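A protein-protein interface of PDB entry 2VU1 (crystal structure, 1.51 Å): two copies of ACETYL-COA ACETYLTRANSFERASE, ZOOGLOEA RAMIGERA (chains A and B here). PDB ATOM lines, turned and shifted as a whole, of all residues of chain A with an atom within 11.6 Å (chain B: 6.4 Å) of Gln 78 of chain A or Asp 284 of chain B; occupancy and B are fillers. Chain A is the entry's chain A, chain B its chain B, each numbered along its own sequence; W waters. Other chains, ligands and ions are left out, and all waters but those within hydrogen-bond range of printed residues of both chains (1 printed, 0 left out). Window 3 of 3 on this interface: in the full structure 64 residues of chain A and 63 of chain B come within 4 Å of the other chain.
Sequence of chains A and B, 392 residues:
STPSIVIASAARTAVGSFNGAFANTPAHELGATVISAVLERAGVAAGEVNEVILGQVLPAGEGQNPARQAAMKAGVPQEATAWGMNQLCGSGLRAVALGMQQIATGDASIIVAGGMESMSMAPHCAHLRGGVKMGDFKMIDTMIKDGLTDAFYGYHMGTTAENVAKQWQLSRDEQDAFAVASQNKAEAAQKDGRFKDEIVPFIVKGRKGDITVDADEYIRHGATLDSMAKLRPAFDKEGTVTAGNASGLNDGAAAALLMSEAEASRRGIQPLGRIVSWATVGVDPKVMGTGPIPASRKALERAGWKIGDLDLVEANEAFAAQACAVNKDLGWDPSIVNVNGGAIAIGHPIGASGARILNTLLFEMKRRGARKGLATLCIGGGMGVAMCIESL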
ATOM      1  N   ALA A  45      -7.114  10.090  17.876  1.00  0.00           N
ATOM      2  CA  ALA A  45      -7.488  11.137  16.965  1.00  0.00           C
ATOM      3  C   ALA A  45      -6.587  11.004  15.746  1.00  0.00           C
ATOM      4  O   ALA A  45      -5.419  10.592  15.885  1.00  0.00           O
ATOM      5  CB  ALA A  45      -7.213  12.500  17.584  1.00  0.00           C
ATOM      6  N   ALA A  46      -7.082  11.385  14.564  1.00  0.00           N
ATOM      7  CA  ALA A  46      -6.311  11.407  13.341  1.00  0.00           C
ATOM      8  C   ALA A  46      -4.991  12.160  13.494  1.00  0.00           C
ATOM      9  O   ALA A  46      -3.951  11.754  12.881  1.00  0.00           O
ATOM     10  CB  ALA A  46      -7.106  11.967  12.166  1.00  0.00           C
ATOM     11  N   GLY A  47      -5.006  13.224  14.329  1.00  0.00           N
ATOM     12  CA  GLY A  47      -3.759  13.976  14.643  1.00  0.00           C
ATOM     13  C   GLY A  47      -2.582  13.218  15.236  1.00  0.00           C
ATOM     14  O   GLY A  47      -1.437  13.603  15.061  1.00  0.00           O
ATOM     15  N   GLU A  48      -2.892  12.061  15.845  1.00  0.00           N
ATOM     16  CA  GLU A  48      -1.923  11.209  16.454  1.00  0.00           C
ATOM     17  C   GLU A  48      -1.300  10.184  15.512  1.00  0.00           C
ATOM     18  O   GLU A  48      -0.299   9.563  15.884  1.00  0.00           O
ATOM     19  CB  GLU A  48      -2.575  10.512  17.603  1.00  0.00           C
ATOM     20  CG  GLU A  48      -3.159  11.482  18.638  1.00  0.00           C
ATOM     21  CD  GLU A  48      -3.818  10.718  19.766  1.00  0.00           C
ATOM     22  OE1 GLU A  48      -3.099  10.304  20.659  1.00  0.00           O
ATOM     23  OE2 GLU A  48      -5.054  10.562  19.824  1.00  0.00           O
ATOM     24  N   VAL A  49      -1.787  10.079  14.309  1.00  0.00           N
ATOM     25  CA  VAL A  49      -1.290   9.015  13.488  1.00  0.00           C
ATOM     26  C   VAL A  49       0.043   9.454  12.901  1.00  0.00           C
ATOM     27  O   VAL A  49       0.156  10.543  12.380  1.00  0.00           O
ATOM     28  CB  VAL A  49      -2.281   8.659  12.375  1.00  0.00           C
ATOM     29  CG1 VAL A  49      -1.682   7.773  11.246  1.00  0.00           C
ATOM     30  CG2 VAL A  49      -3.543   8.143  12.905  1.00  0.00           C
ATOM     31  N   ASN A  50       1.026   8.585  12.893  1.00  0.00           N
ATOM     32  CA  ASN A  50       2.321   8.906  12.322  1.00  0.00           C
ATOM     33  C   ASN A  50       2.435   8.500  10.820  1.00  0.00           C
ATOM     34  O   ASN A  50       3.026   9.241  10.010  1.00  0.00           O
ATOM     35  CB  ASN A  50       3.483   8.333  13.215  1.00  0.00           C
ATOM     36  CG  ASN A  50       3.491   8.803  14.560  1.00  0.00           C
ATOM     37  OD1 ASN A  50       3.495   7.992  15.456  1.00  0.00           O
ATOM     38  ND2 ASN A  50       3.540  10.127  14.762  1.00  0.00           N
ATOM     39  N   GLU A  51       1.949   7.302  10.487  1.00  0.00           N
ATOM     40  CA  GLU A  51       2.039   6.797   9.150  1.00  0.00           C
ATOM     41  C   GLU A  51       0.891   5.859   8.832  1.00  0.00           C
ATOM     42  O   GLU A  51       0.341   5.244   9.745  1.00  0.00           O
ATOM     43  CB  GLU A  51       3.376   6.140   8.948  1.00  0.00           C
ATOM     44  CG  GLU A  51       3.598   5.843   7.507  1.00  0.00           C
ATOM     45  CD  GLU A  51       5.057   5.581   7.222  1.00  0.00           C
ATOM     46  OE1 GLU A  51       5.554   4.592   7.801  1.00  0.00           O
ATOM     47  OE2 GLU A  51       5.675   6.341   6.447  1.00  0.00           O
ATOM     48  N   VAL A  52       0.424   5.925   7.612  1.00  0.00           N
ATOM     49  CA  VAL A  52      -0.595   5.031   7.040  1.00  0.00           C
ATOM     50  C   VAL A  52       0.104   4.140   5.936  1.00  0.00           C
ATOM     51  O   VAL A  52       0.794   4.656   5.058  1.00  0.00           O
ATOM     52  CB  VAL A  52      -1.775   5.855   6.387  1.00  0.00           C
ATOM     53  CG1 VAL A  52      -2.746   4.921   5.571  1.00  0.00           C
ATOM     54  CG2 VAL A  52      -2.476   6.700   7.441  1.00  0.00           C
ATOM     55  N   GLN A  64      -1.638  10.010  -7.666  1.00  0.00           N
ATOM     56  CA  GLN A  64      -0.462   9.862  -6.827  1.00  0.00           C
ATOM     57  C   GLN A  64      -0.769   9.242  -5.538  1.00  0.00           C
ATOM     58  O   GLN A  64      -1.628   9.751  -4.791  1.00  0.00           O
ATOM     59  CB  GLN A  64       0.242  11.243  -6.559  1.00  0.00           C
ATOM     60  CG  GLN A  64       1.303  11.673  -7.541  1.00  0.00           C
ATOM     61  CD  GLN A  64       2.050  12.939  -7.087  1.00  0.00           C
ATOM     62  OE1 GLN A  64       1.602  13.618  -6.204  1.00  0.00           O
ATOM     63  NE2 GLN A  64       3.171  13.250  -7.746  1.00  0.00           N
ATOM     64  N   ASN A  65      -0.051   8.136  -5.276  1.00  0.00           N
ATOM     65  CA  ASN A  65       0.017   7.490  -3.975  1.00  0.00           C
ATOM     66  C   ASN A  65      -1.310   7.449  -3.215  1.00  0.00           C
ATOM     67  O   ASN A  65      -1.580   8.259  -2.327  1.00  0.00           O
ATOM     68  CB  ASN A  65       1.078   8.199  -3.125  1.00  0.00           C
ATOM     69  CG  ASN A  65       1.346   7.531  -1.775  1.00  0.00           C
ATOM     70  OD1 ASN A  65       0.928   6.385  -1.490  1.00  0.00           O
ATOM     71  ND2 ASN A  65       2.073   8.236  -0.925  1.00  0.00           N
ATOM     72  N   ALA A  67      -2.617   5.751  -0.982  1.00  0.00           N
ATOM     73  CA  ALA A  67      -2.492   5.634   0.471  1.00  0.00           C
ATOM     74  C   ALA A  67      -2.582   7.027   1.113  1.00  0.00           C
ATOM     75  O   ALA A  67      -3.235   7.254   2.163  1.00  0.00           O
ATOM     76  CB  ALA A  67      -1.201   4.952   0.937  1.00  0.00           C
ATOM     77  N   ARG A  68      -1.825   7.947   0.567  1.00  0.00           N
ATOM     78  CA  ARG A  68      -1.808   9.342   1.062  1.00  0.00           C
ATOM     79  C   ARG A  68      -3.160   9.993   0.857  1.00  0.00           C
ATOM     80  O   ARG A  68      -3.615  10.845   1.645  1.00  0.00           O
ATOM     81  CB  ARG A  68      -0.755  10.167   0.281  1.00  0.00           C
ATOM     82  CG  ARG A  68      -0.575  11.654   0.745  1.00  0.00           C
ATOM     83  CD  ARG A  68      -0.073  11.786   2.127  1.00  0.00           C
ATOM     84  NE  ARG A  68       0.441  13.181   2.201  1.00  0.00           N
ATOM     85  CZ  ARG A  68       0.928  13.712   3.289  1.00  0.00           C
ATOM     86  NH1 ARG A  68       0.878  13.055   4.403  1.00  0.00           N
ATOM     87  NH2 ARG A  68       1.437  14.908   3.221  1.00  0.00           N
ATOM     88  N   GLN A  69      -3.768   9.686  -0.289  1.00  0.00           N
ATOM     89  CA  GLN A  69      -5.113  10.182  -0.574  1.00  0.00           C
ATOM     90  C   GLN A  69      -6.129   9.689   0.449  1.00  0.00           C
ATOM     91  O   GLN A  69      -6.953  10.510   0.879  1.00  0.00           O
ATOM     92  CB  GLN A  69      -5.589   9.784  -1.953  1.00  0.00           C
ATOM     93  CG  GLN A  69      -4.794  10.358  -3.141  1.00  0.00           C
ATOM     94  CD  GLN A  69      -5.387  10.027  -4.481  1.00  0.00           C
ATOM     95  OE1 GLN A  69      -6.561  10.303  -4.749  1.00  0.00           O
ATOM     96  NE2 GLN A  69      -4.556   9.480  -5.338  1.00  0.00           N
ATOM     97  N   ALA A  70      -6.044   8.433   0.866  1.00  0.00           N
ATOM     98  CA  ALA A  70      -6.889   7.856   1.915  1.00  0.00           C
ATOM     99  C   ALA A  70      -6.616   8.547   3.249  1.00  0.00           C
ATOM    100  O   ALA A  70      -7.526   8.940   3.928  1.00  0.00           O
ATOM    101  CB  ALA A  70      -6.652   6.415   2.006  1.00  0.00           C
ATOM    102  N   ALA A  71      -5.378   8.762   3.540  1.00  0.00           N
ATOM    103  CA  ALA A  71      -4.954   9.332   4.842  1.00  0.00           C
ATOM    104  C   ALA A  71      -5.468  10.763   4.904  1.00  0.00           C
ATOM    105  O   ALA A  71      -6.115  11.146   5.821  1.00  0.00           O
ATOM    106  CB  ALA A  71      -3.456   9.345   4.948  1.00  0.00           C
ATOM    107  N   MET A  72      -5.307  11.531   3.828  1.00  0.00           N
ATOM    108  CA  MET A  72      -5.712  12.913   3.838  1.00  0.00           C
ATOM    109  C   MET A  72      -7.217  13.085   3.933  1.00  0.00           C
ATOM    110  O   MET A  72      -7.712  13.915   4.708  1.00  0.00           O
ATOM    111  CB  MET A  72      -5.120  13.575   2.627  1.00  0.00           C
ATOM    112  CG  MET A  72      -3.585  13.746   2.791  1.00  0.00           C
ATOM    113  SD  MET A  72      -3.031  15.047   3.943  1.00  0.00           S
ATOM    114  CE  MET A  72      -3.167  16.462   2.812  1.00  0.00           C
ATOM    115  N   LYS A  73      -7.935  12.186   3.283  1.00  0.00           N
ATOM    116  CA  LYS A  73      -9.399  12.268   3.259  1.00  0.00           C
ATOM    117  C   LYS A  73      -9.879  11.960   4.667  1.00  0.00           C
ATOM    118  O   LYS A  73     -10.878  12.555   5.151  1.00  0.00           O
ATOM    119  CB  LYS A  73      -9.948  11.318   2.200  1.00  0.00           C
ATOM    120  CG  LYS A  73     -11.491  11.234   2.036  1.00  0.00           C
ATOM    121  CD  LYS A  73     -12.186  12.540   1.906  1.00  0.00           C
ATOM    122  CE  LYS A  73     -13.724  12.334   1.715  1.00  0.00           C
ATOM    123  NZ  LYS A  73     -14.171  11.952   0.335  1.00  0.00           N
ATOM    124  N   ALA A  74      -9.189  11.066   5.360  1.00  0.00           N
ATOM    125  CA  ALA A  74      -9.528  10.711   6.699  1.00  0.00           C
ATOM    126  C   ALA A  74      -9.131  11.757   7.739  1.00  0.00           C
ATOM    127  O   ALA A  74      -9.392  11.584   8.948  1.00  0.00           O
ATOM    128  CB  ALA A  74      -8.943   9.321   7.058  1.00  0.00           C
ATOM    129  N   GLY A  75      -8.494  12.845   7.322  1.00  0.00           N
ATOM    130  CA  GLY A  75      -8.080  13.891   8.302  1.00  0.00           C
ATOM    131  C   GLY A  75      -6.745  13.631   8.978  1.00  0.00           C
ATOM    132  O   GLY A  75      -6.345  14.314   9.919  1.00  0.00           O
ATOM    133  N   VAL A  76      -5.979  12.637   8.479  1.00  0.00           N
ATOM    134  CA  VAL A  76      -4.671  12.415   8.996  1.00  0.00           C
ATOM    135  C   VAL A  76      -3.844  13.637   8.534  1.00  0.00           C
ATOM    136  O   VAL A  76      -3.942  14.108   7.409  1.00  0.00           O
ATOM    137  CB  VAL A  76      -4.018  11.079   8.463  1.00  0.00           C
ATOM    138  CG1 VAL A  76      -2.562  10.906   8.985  1.00  0.00           C
ATOM    139  CG2 VAL A  76      -4.927   9.857   8.777  1.00  0.00           C
ATOM    140  N   PRO A  77      -3.042  14.172   9.456  1.00  0.00           N
ATOM    141  CA  PRO A  77      -2.375  15.415   9.146  1.00  0.00           C
ATOM    142  C   PRO A  77      -1.344  15.329   8.028  1.00  0.00           C
ATOM    143  O   PRO A  77      -0.785  14.285   7.744  1.00  0.00           O
ATOM    144  CB  PRO A  77      -1.675  15.765  10.466  1.00  0.00           C
ATOM    145  CG  PRO A  77      -1.604  14.635  11.206  1.00  0.00           C
ATOM    146  CD  PRO A  77      -2.757  13.775  10.852  1.00  0.00           C
ATOM    147  N   GLN A  78      -1.102  16.476   7.447  1.00  0.00           N
ATOM    148  CA  GLN A  78      -0.112  16.508   6.370  1.00  0.00           C
ATOM    149  C   GLN A  78       1.256  16.125   6.915  1.00  0.00           C
ATOM    150  O   GLN A  78       2.125  15.698   6.143  1.00  0.00           O
ATOM    151  CB  GLN A  78      -0.090  17.844   5.589  1.00  0.00           C
ATOM    152  CG  GLN A  78       0.371  18.975   6.389  1.00  0.00           C
ATOM    153  CD  GLN A  78       0.065  20.329   5.761  1.00  0.00           C
ATOM    154  OE1 GLN A  78       0.821  21.261   5.931  1.00  0.00           O
ATOM    155  NE2 GLN A  78      -1.053  20.426   5.058  1.00  0.00           N
ATOM    156  N   GLU A  79       1.514  16.272   8.224  1.00  0.00           N
ATOM    157  CA  GLU A  79       2.822  15.960   8.736  1.00  0.00           C
ATOM    158  C   GLU A  79       3.126  14.479   8.861  1.00  0.00           C
ATOM    159  O   GLU A  79       4.307  14.098   9.004  1.00  0.00           O
ATOM    160  CB  GLU A  79       2.953  16.570  10.043  1.00  0.00           C
ATOM    161  CG  GLU A  79       3.015  18.090  10.066  1.00  0.00           C
ATOM    162  CD  GLU A  79       1.641  18.831  10.037  1.00  0.00           C
ATOM    163  OE1 GLU A  79       0.556  18.212  10.161  1.00  0.00           O
ATOM    164  OE2 GLU A  79       1.671  20.069   9.813  1.00  0.00           O
ATOM    165  N   ALA A  80       2.042  13.670   8.877  1.00  0.00           N
ATOM    166  CA  ALA A  80       2.153  12.211   8.868  1.00  0.00           C
ATOM    167  C   ALA A  80       2.640  11.842   7.471  1.00  0.00           C
ATOM    168  O   ALA A  80       2.828  12.683   6.552  1.00  0.00           O
ATOM    169  CB  ALA A  80       0.841  11.563   9.206  1.00  0.00           C
ATOM    170  N   THR A  81       2.961  10.565   7.313  1.00  0.00           N
ATOM    171  CA  THR A  81       3.328  10.103   6.017  1.00  0.00           C
ATOM    172  C   THR A  81       2.422   8.909   5.630  1.00  0.00           C
ATOM    173  O   THR A  81       1.649   8.430   6.427  1.00  0.00           O
ATOM    174  CB  THR A  81       4.818   9.654   5.933  1.00  0.00           C
ATOM    175  OG1 THR A  81       5.080   8.756   7.011  1.00  0.00           O
ATOM    176  CG2 THR A  81       5.760  10.822   5.980  1.00  0.00           C
ATOM    177  N   ALA A  82       2.476   8.452   4.393  1.00  0.00           N
ATOM    178  CA  ALA A  82       1.582   7.373   3.864  1.00  0.00           C
ATOM    179  C   ALA A  82       2.292   6.785   2.666  1.00  0.00           C
ATOM    180  O   ALA A  82       2.980   7.456   1.973  1.00  0.00           O
ATOM    181  CB  ALA A  82       0.252   7.938   3.418  1.00  0.00           C
ATOM    182  N   TRP A  83       2.098   5.506   2.432  1.00  0.00           N
ATOM    183  CA  TRP A  83       2.669   4.838   1.260  1.00  0.00           C
ATOM    184  C   TRP A  83       1.937   3.540   1.049  1.00  0.00           C
ATOM    185  O   TRP A  83       1.185   3.043   1.923  1.00  0.00           O
ATOM    186  CB  TRP A  83       4.130   4.618   1.509  1.00  0.00           C
ATOM    187  CG  TRP A  83       4.566   3.905   2.776  1.00  0.00           C
ATOM    188  CD1 TRP A  83       4.701   4.462   4.072  1.00  0.00           C
ATOM    189  CD2 TRP A  83       4.994   2.525   2.943  1.00  0.00           C
ATOM    190  NE1 TRP A  83       5.161   3.553   4.935  1.00  0.00           N
ATOM    191  CE2 TRP A  83       5.428   2.384   4.276  1.00  0.00           C
ATOM    192  CE3 TRP A  83       5.111   1.435   2.087  1.00  0.00           C
ATOM    193  CZ2 TRP A  83       5.872   1.162   4.791  1.00  0.00           C
ATOM    194  CZ3 TRP A  83       5.563   0.242   2.585  1.00  0.00           C
ATOM    195  CH2 TRP A  83       5.997   0.124   3.906  1.00  0.00           C
ATOM    196  N   TYR B 153      -4.670  18.962  -5.469  1.00  0.00           N
ATOM    197  CA  TYR B 153      -4.843  20.231  -6.174  1.00  0.00           C
ATOM    198  C   TYR B 153      -5.013  20.046  -7.668  1.00  0.00           C
ATOM    199  O   TYR B 153      -5.460  20.968  -8.357  1.00  0.00           O
ATOM    200  CB  TYR B 153      -3.644  21.102  -5.856  1.00  0.00           C
ATOM    201  CG  TYR B 153      -3.654  21.522  -4.414  1.00  0.00           C
ATOM    202  CD1 TYR B 153      -4.397  22.619  -4.017  1.00  0.00           C
ATOM    203  CD2 TYR B 153      -2.979  20.804  -3.431  1.00  0.00           C
ATOM    204  CE1 TYR B 153      -4.425  23.021  -2.687  1.00  0.00           C
ATOM    205  CE2 TYR B 153      -3.005  21.194  -2.105  1.00  0.00           C
ATOM    206  CZ  TYR B 153      -3.744  22.301  -1.740  1.00  0.00           C
ATOM    207  OH  TYR B 153      -3.811  22.719  -0.441  1.00  0.00           O
ATOM    208  N   VAL B 281       9.000  12.422   6.802  1.00  0.00           N
ATOM    209  CA  VAL B 281       8.130  13.465   7.355  1.00  0.00           C
ATOM    210  C   VAL B 281       7.211  14.001   6.302  1.00  0.00           C
ATOM    211  O   VAL B 281       7.563  14.029   5.141  1.00  0.00           O
ATOM    212  CB  VAL B 281       8.892  14.652   8.035  1.00  0.00           C
ATOM    213  CG1 VAL B 281       7.920  15.700   8.646  1.00  0.00           C
ATOM    214  CG2 VAL B 281       9.748  14.048   9.146  1.00  0.00           C
ATOM    215  N   GLY B 282       6.032  14.486   6.725  1.00  0.00           N
ATOM    216  CA  GLY B 282       5.111  15.083   5.774  1.00  0.00           C
ATOM    217  C   GLY B 282       5.204  16.616   5.845  1.00  0.00           C
ATOM    218  O   GLY B 282       5.594  17.189   6.851  1.00  0.00           O
ATOM    219  N   VAL B 283       4.811  17.239   4.755  1.00  0.00           N
ATOM    220  CA  VAL B 283       4.664  18.718   4.616  1.00  0.00           C
ATOM    221  C   VAL B 283       3.387  19.007   3.720  1.00  0.00           C
ATOM    222  O   VAL B 283       2.711  18.068   3.191  1.00  0.00           O
ATOM    223  CB  VAL B 283       5.960  19.345   3.948  1.00  0.00           C
ATOM    224  CG1 VAL B 283       7.181  18.913   4.725  1.00  0.00           C
ATOM    225  CG2 VAL B 283       6.084  18.910   2.526  1.00  0.00           C
ATOM    226  N   ASP B 284       3.070  20.278   3.552  1.00  0.00           N
ATOM    227  CA  ASP B 284       1.966  20.676   2.671  1.00  0.00           C
ATOM    228  C   ASP B 284       2.234  20.154   1.271  1.00  0.00           C
ATOM    229  O   ASP B 284       3.280  20.448   0.729  1.00  0.00           O
ATOM    230  CB  ASP B 284       1.761  22.171   2.648  1.00  0.00           C
ATOM    231  CG  ASP B 284       0.374  22.539   2.147  1.00  0.00           C
ATOM    232  OD1 ASP B 284      -0.001  22.156   1.006  1.00  0.00           O
ATOM    233  OD2 ASP B 284      -0.388  23.126   2.951  1.00  0.00           O
ATOM    234  N   PRO B 285       1.287  19.433   0.651  1.00  0.00           N
ATOM    235  CA  PRO B 285       1.424  19.074  -0.771  1.00  0.00           C
ATOM    236  C   PRO B 285       1.755  20.231  -1.716  1.00  0.00           C
ATOM    237  O   PRO B 285       2.438  20.006  -2.763  1.00  0.00           O
ATOM    238  CB  PRO B 285       0.053  18.532  -1.164  1.00  0.00           C
ATOM    239  CG  PRO B 285      -0.608  18.120   0.110  1.00  0.00           C
ATOM    240  CD  PRO B 285       0.043  18.906   1.231  1.00  0.00           C
ATOM    241  N   LYS B 286       1.272  21.426  -1.403  1.00  0.00           N
ATOM    242  CA  LYS B 286       1.493  22.577  -2.290  1.00  0.00           C
ATOM    243  C   LYS B 286       2.950  22.980  -2.393  1.00  0.00           C
ATOM    244  O   LYS B 286       3.341  23.645  -3.332  1.00  0.00           O
ATOM    245  CB  LYS B 286       0.710  23.794  -1.799  1.00  0.00           C
ATOM    246  CG  LYS B 286      -0.802  23.600  -1.766  1.00  0.00           C
ATOM    247  CD  LYS B 286      -1.568  24.959  -1.632  1.00  0.00           C
ATOM    248  CE  LYS B 286      -0.907  25.889  -0.632  1.00  0.00           C
ATOM    249  NZ  LYS B 286      -0.623  25.194   0.649  1.00  0.00           N
ATOM    250  N   VAL B 287       3.724  22.674  -1.365  1.00  0.00           N
ATOM    251  CA  VAL B 287       5.161  22.924  -1.368  1.00  0.00           C
ATOM    252  C   VAL B 287       5.867  21.607  -1.003  1.00  0.00           C
ATOM    253  O   VAL B 287       6.698  21.480  -0.070  1.00  0.00           O
ATOM    254  CB  VAL B 287       5.484  24.074  -0.398  1.00  0.00           C
ATOM    255  CG1 VAL B 287       4.994  25.412  -0.989  1.00  0.00           C
ATOM    256  CG2 VAL B 287       4.947  23.787   1.052  1.00  0.00           C
ATOM    257  N   MET B 288       5.546  20.570  -1.757  1.00  0.00           N
ATOM    258  CA  MET B 288       6.132  19.254  -1.466  1.00  0.00           C
ATOM    259  C   MET B 288       7.669  19.250  -1.582  1.00  0.00           C
ATOM    260  O   MET B 288       8.316  18.395  -0.965  1.00  0.00           O
ATOM    261  CB  MET B 288       5.549  18.244  -2.429  1.00  0.00           C
ATOM    262  CG  MET B 288       5.896  18.493  -3.932  1.00  0.00           C
ATOM    263  SD  MET B 288       7.353  17.456  -4.381  1.00  0.00           S
ATOM    264  CE  MET B 288       7.765  18.066  -6.043  1.00  0.00           C
ATOM    265  N   GLY B 289       8.212  20.199  -2.350  1.00  0.00           N
ATOM    266  CA  GLY B 289       9.671  20.314  -2.619  1.00  0.00           C
ATOM    267  C   GLY B 289      10.426  20.591  -1.368  1.00  0.00           C
ATOM    268  O   GLY B 289      11.637  20.396  -1.326  1.00  0.00           O
ATOM    269  N   THR B 290       9.681  21.020  -0.337  1.00  0.00           N
ATOM    270  CA  THR B 290      10.240  21.355   0.968  1.00  0.00           C
ATOM    271  C   THR B 290      10.439  20.134   1.914  1.00  0.00           C
ATOM    272  O   THR B 290      11.044  20.274   2.981  1.00  0.00           O
ATOM    273  CB  THR B 290       9.474  22.469   1.698  1.00  0.00           C
ATOM    274  OG1 THR B 290       8.195  21.975   2.115  1.00  0.00           O
ATOM    275  CG2 THR B 290       9.393  23.739   0.860  1.00  0.00           C
ATOM    276  N   GLY B 381       2.843  14.842  -3.097  1.00  0.00           N
ATOM    277  CA  GLY B 381       1.840  14.751  -2.042  1.00  0.00           C
ATOM    278  C   GLY B 381       2.333  15.253  -0.726  1.00  0.00           C
ATOM    279  O   GLY B 381       1.615  15.108   0.262  1.00  0.00           O
ATOM    280  N   GLY B 382       3.520  15.888  -0.705  1.00  0.00           N
ATOM    281  CA  GLY B 382       4.006  16.538   0.535  1.00  0.00           C
ATOM    282  C   GLY B 382       4.704  15.623   1.508  1.00  0.00           C
ATOM    283  O   GLY B 382       4.266  15.513   2.672  1.00  0.00           O
ATOM    284  N   MET B 383       5.818  15.044   1.095  1.00  0.00           N
ATOM    285  CA  MET B 383       6.623  14.336   2.071  1.00  0.00           C
ATOM    286  C   MET B 383       8.112  14.516   1.762  1.00  0.00           C
ATOM    287  O   MET B 383       8.504  15.049   0.697  1.00  0.00           O
ATOM    288  CB  MET B 383       6.248  12.847   2.180  1.00  0.00           C
ATOM    289  CG  MET B 383       4.829  12.542   2.617  1.00  0.00           C
ATOM    290  SD  MET B 383       4.452  10.769   2.443  1.00  0.00           S
ATOM    291  CE  MET B 383       3.907  10.813   0.758  1.00  0.00           C
HETATM  292  O   HOH W   1       0.425  23.880   5.445  1.00  0.00           O
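The guanidinium group (NH2) of Arg 68 of chain A lies within hydrogen-bond range of the backbone carbonyl oxygen (O) of Val 283 of chain B (3.4 Å). The guanidinium group of Arg 68 of chain A lies within hydrogen-bond range of the backbone carbonyl oxygen of Gly 381 of chain B, at 3.0 Å. The backbone carbonyl oxygen (O) of Gly 382 of chain B sits at hydrogen-bond distance from the guanidinium group (NH2) of Arg 68 of chain A, 2.9 Å away. The backbone carbonyl oxygen (O) of Gln 78 of chain A lies within hydrogen-bond range of the backbone NH (N) of Val 283 of chain B, at 3.4 Å. OE1 of Gln 78 of chain A is in hydrogen-bond range of N of Asp 284 of chain B, 3.4 Å away. The backbone NH (N) of Gly 282 of chain B sits at hydrogen-bond distance from the backbone carbonyl oxygen (O) of Glu 79 of chain A (2.9 Å). The backbone NH (N) of Ala 82 of chain A lies within hydrogen-bond range of the side-chain sulfur (SD) of Met 383 of chain B.
N of Thr 81 of chain A is in hydrogen-bond range of O of Asn 50 of chain A. The backbone carbonyl oxygen (O) of Thr 81 of chain A sits at hydrogen-bond distance from the backbone NH (N) of Val 52 of chain A (3.0 Å). O of Gln 78 of chain A is in hydrogen-bond range of NH2 of Arg 68 of chain A, 3.1 Å away.
Gln 64 of chain A touches Gly 381 of chain B (OE1 to N, 3.6 Å). ND2 of Asn 65 of chain A touches CE of Met 383 of chain B (3.6 Å). CA of Gly 282 of chain B touches O of Gln 78 of chain A (3.1 Å). Glu 79 of chain A touches Val 281 of chain B (O to C, 3.97 Å). O of Ala 80 of chain A touches CA of Gly 282 of chain B (3.4 Å). CG2 of Thr 81 of chain A touches C of Val 281 of chain B, at 3.5 Å. Gly 282 of chain B touches Thr 81 of chain A.
Gln 78 of chain A touches just these residues of chain B: Gly 282 (3.1 Å), Val 283 (3.4 Å) and Asp 284 (3.4 Å). Printed residues of chain A within 4 Å of Asp 284 of chain B: Gln 78 (3.4 Å). Of chain A, only Arg 68 and Gln 78 come within 4 Å of Val 283 of chain B. No residue of chain A comes within 4 Å of Pro 285 of chain B. No residue of chain A comes within 4 Å of Val 287 of chain B. Met 383 of chain B touches just these residues of chain A: Asn 65 (3.6 Å), Thr 81 (3.7 Å) and Ala 82 (3.6 Å). Printed residues of chain B within 4 Å of Thr 81 of chain A: Val 281 (3.5 Å), Gly 282 (3.7 Å) and Met 383 (3.7 Å). Of the printed residues of chain B, Ala 80 of chain A touches Gly 282. Of the printed residues of chain B, Gln 64 of chain A touches Gly 381. Gln 69 of chain A touches none of the printed residues of chain B. The nearest residue of chain B that does not touch Gln 78 of chain A is Gly 382 of chain B (4.1 Å). The nearest residue of chain A that does not touch Asp 284 of chain B is Arg 68 of chain A (5.6 Å). The nearest printed residue of chain B that does not touch Arg 68 of chain A is Met 383 of chain B (4.1 Å).
Printed residues of chain A that touch a printed residue of chain B: Gln 64, Asn 65, Arg 68, Gln 78, Glu 79, Ala 80, Thr 81 and Ala 82. Hydrophobic or aromatic side chains of chain B that line the printed part of chain A: Val 281 and Met 383. Among the printed residues, no Asp or Glu carboxylate lies within 4 Å of a Lys or Arg side-chain nitrogen of the other chain.
No position is printed for both chains. Of the 15 pairs that touch across the chains among the printed residues, none has its exchanged pair printed and touching as well.
Water W1 bridges OE1 of Gln 78 of chain A (2.7 Å) and OD2 of Asp 284 of chain B (2.7 Å).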
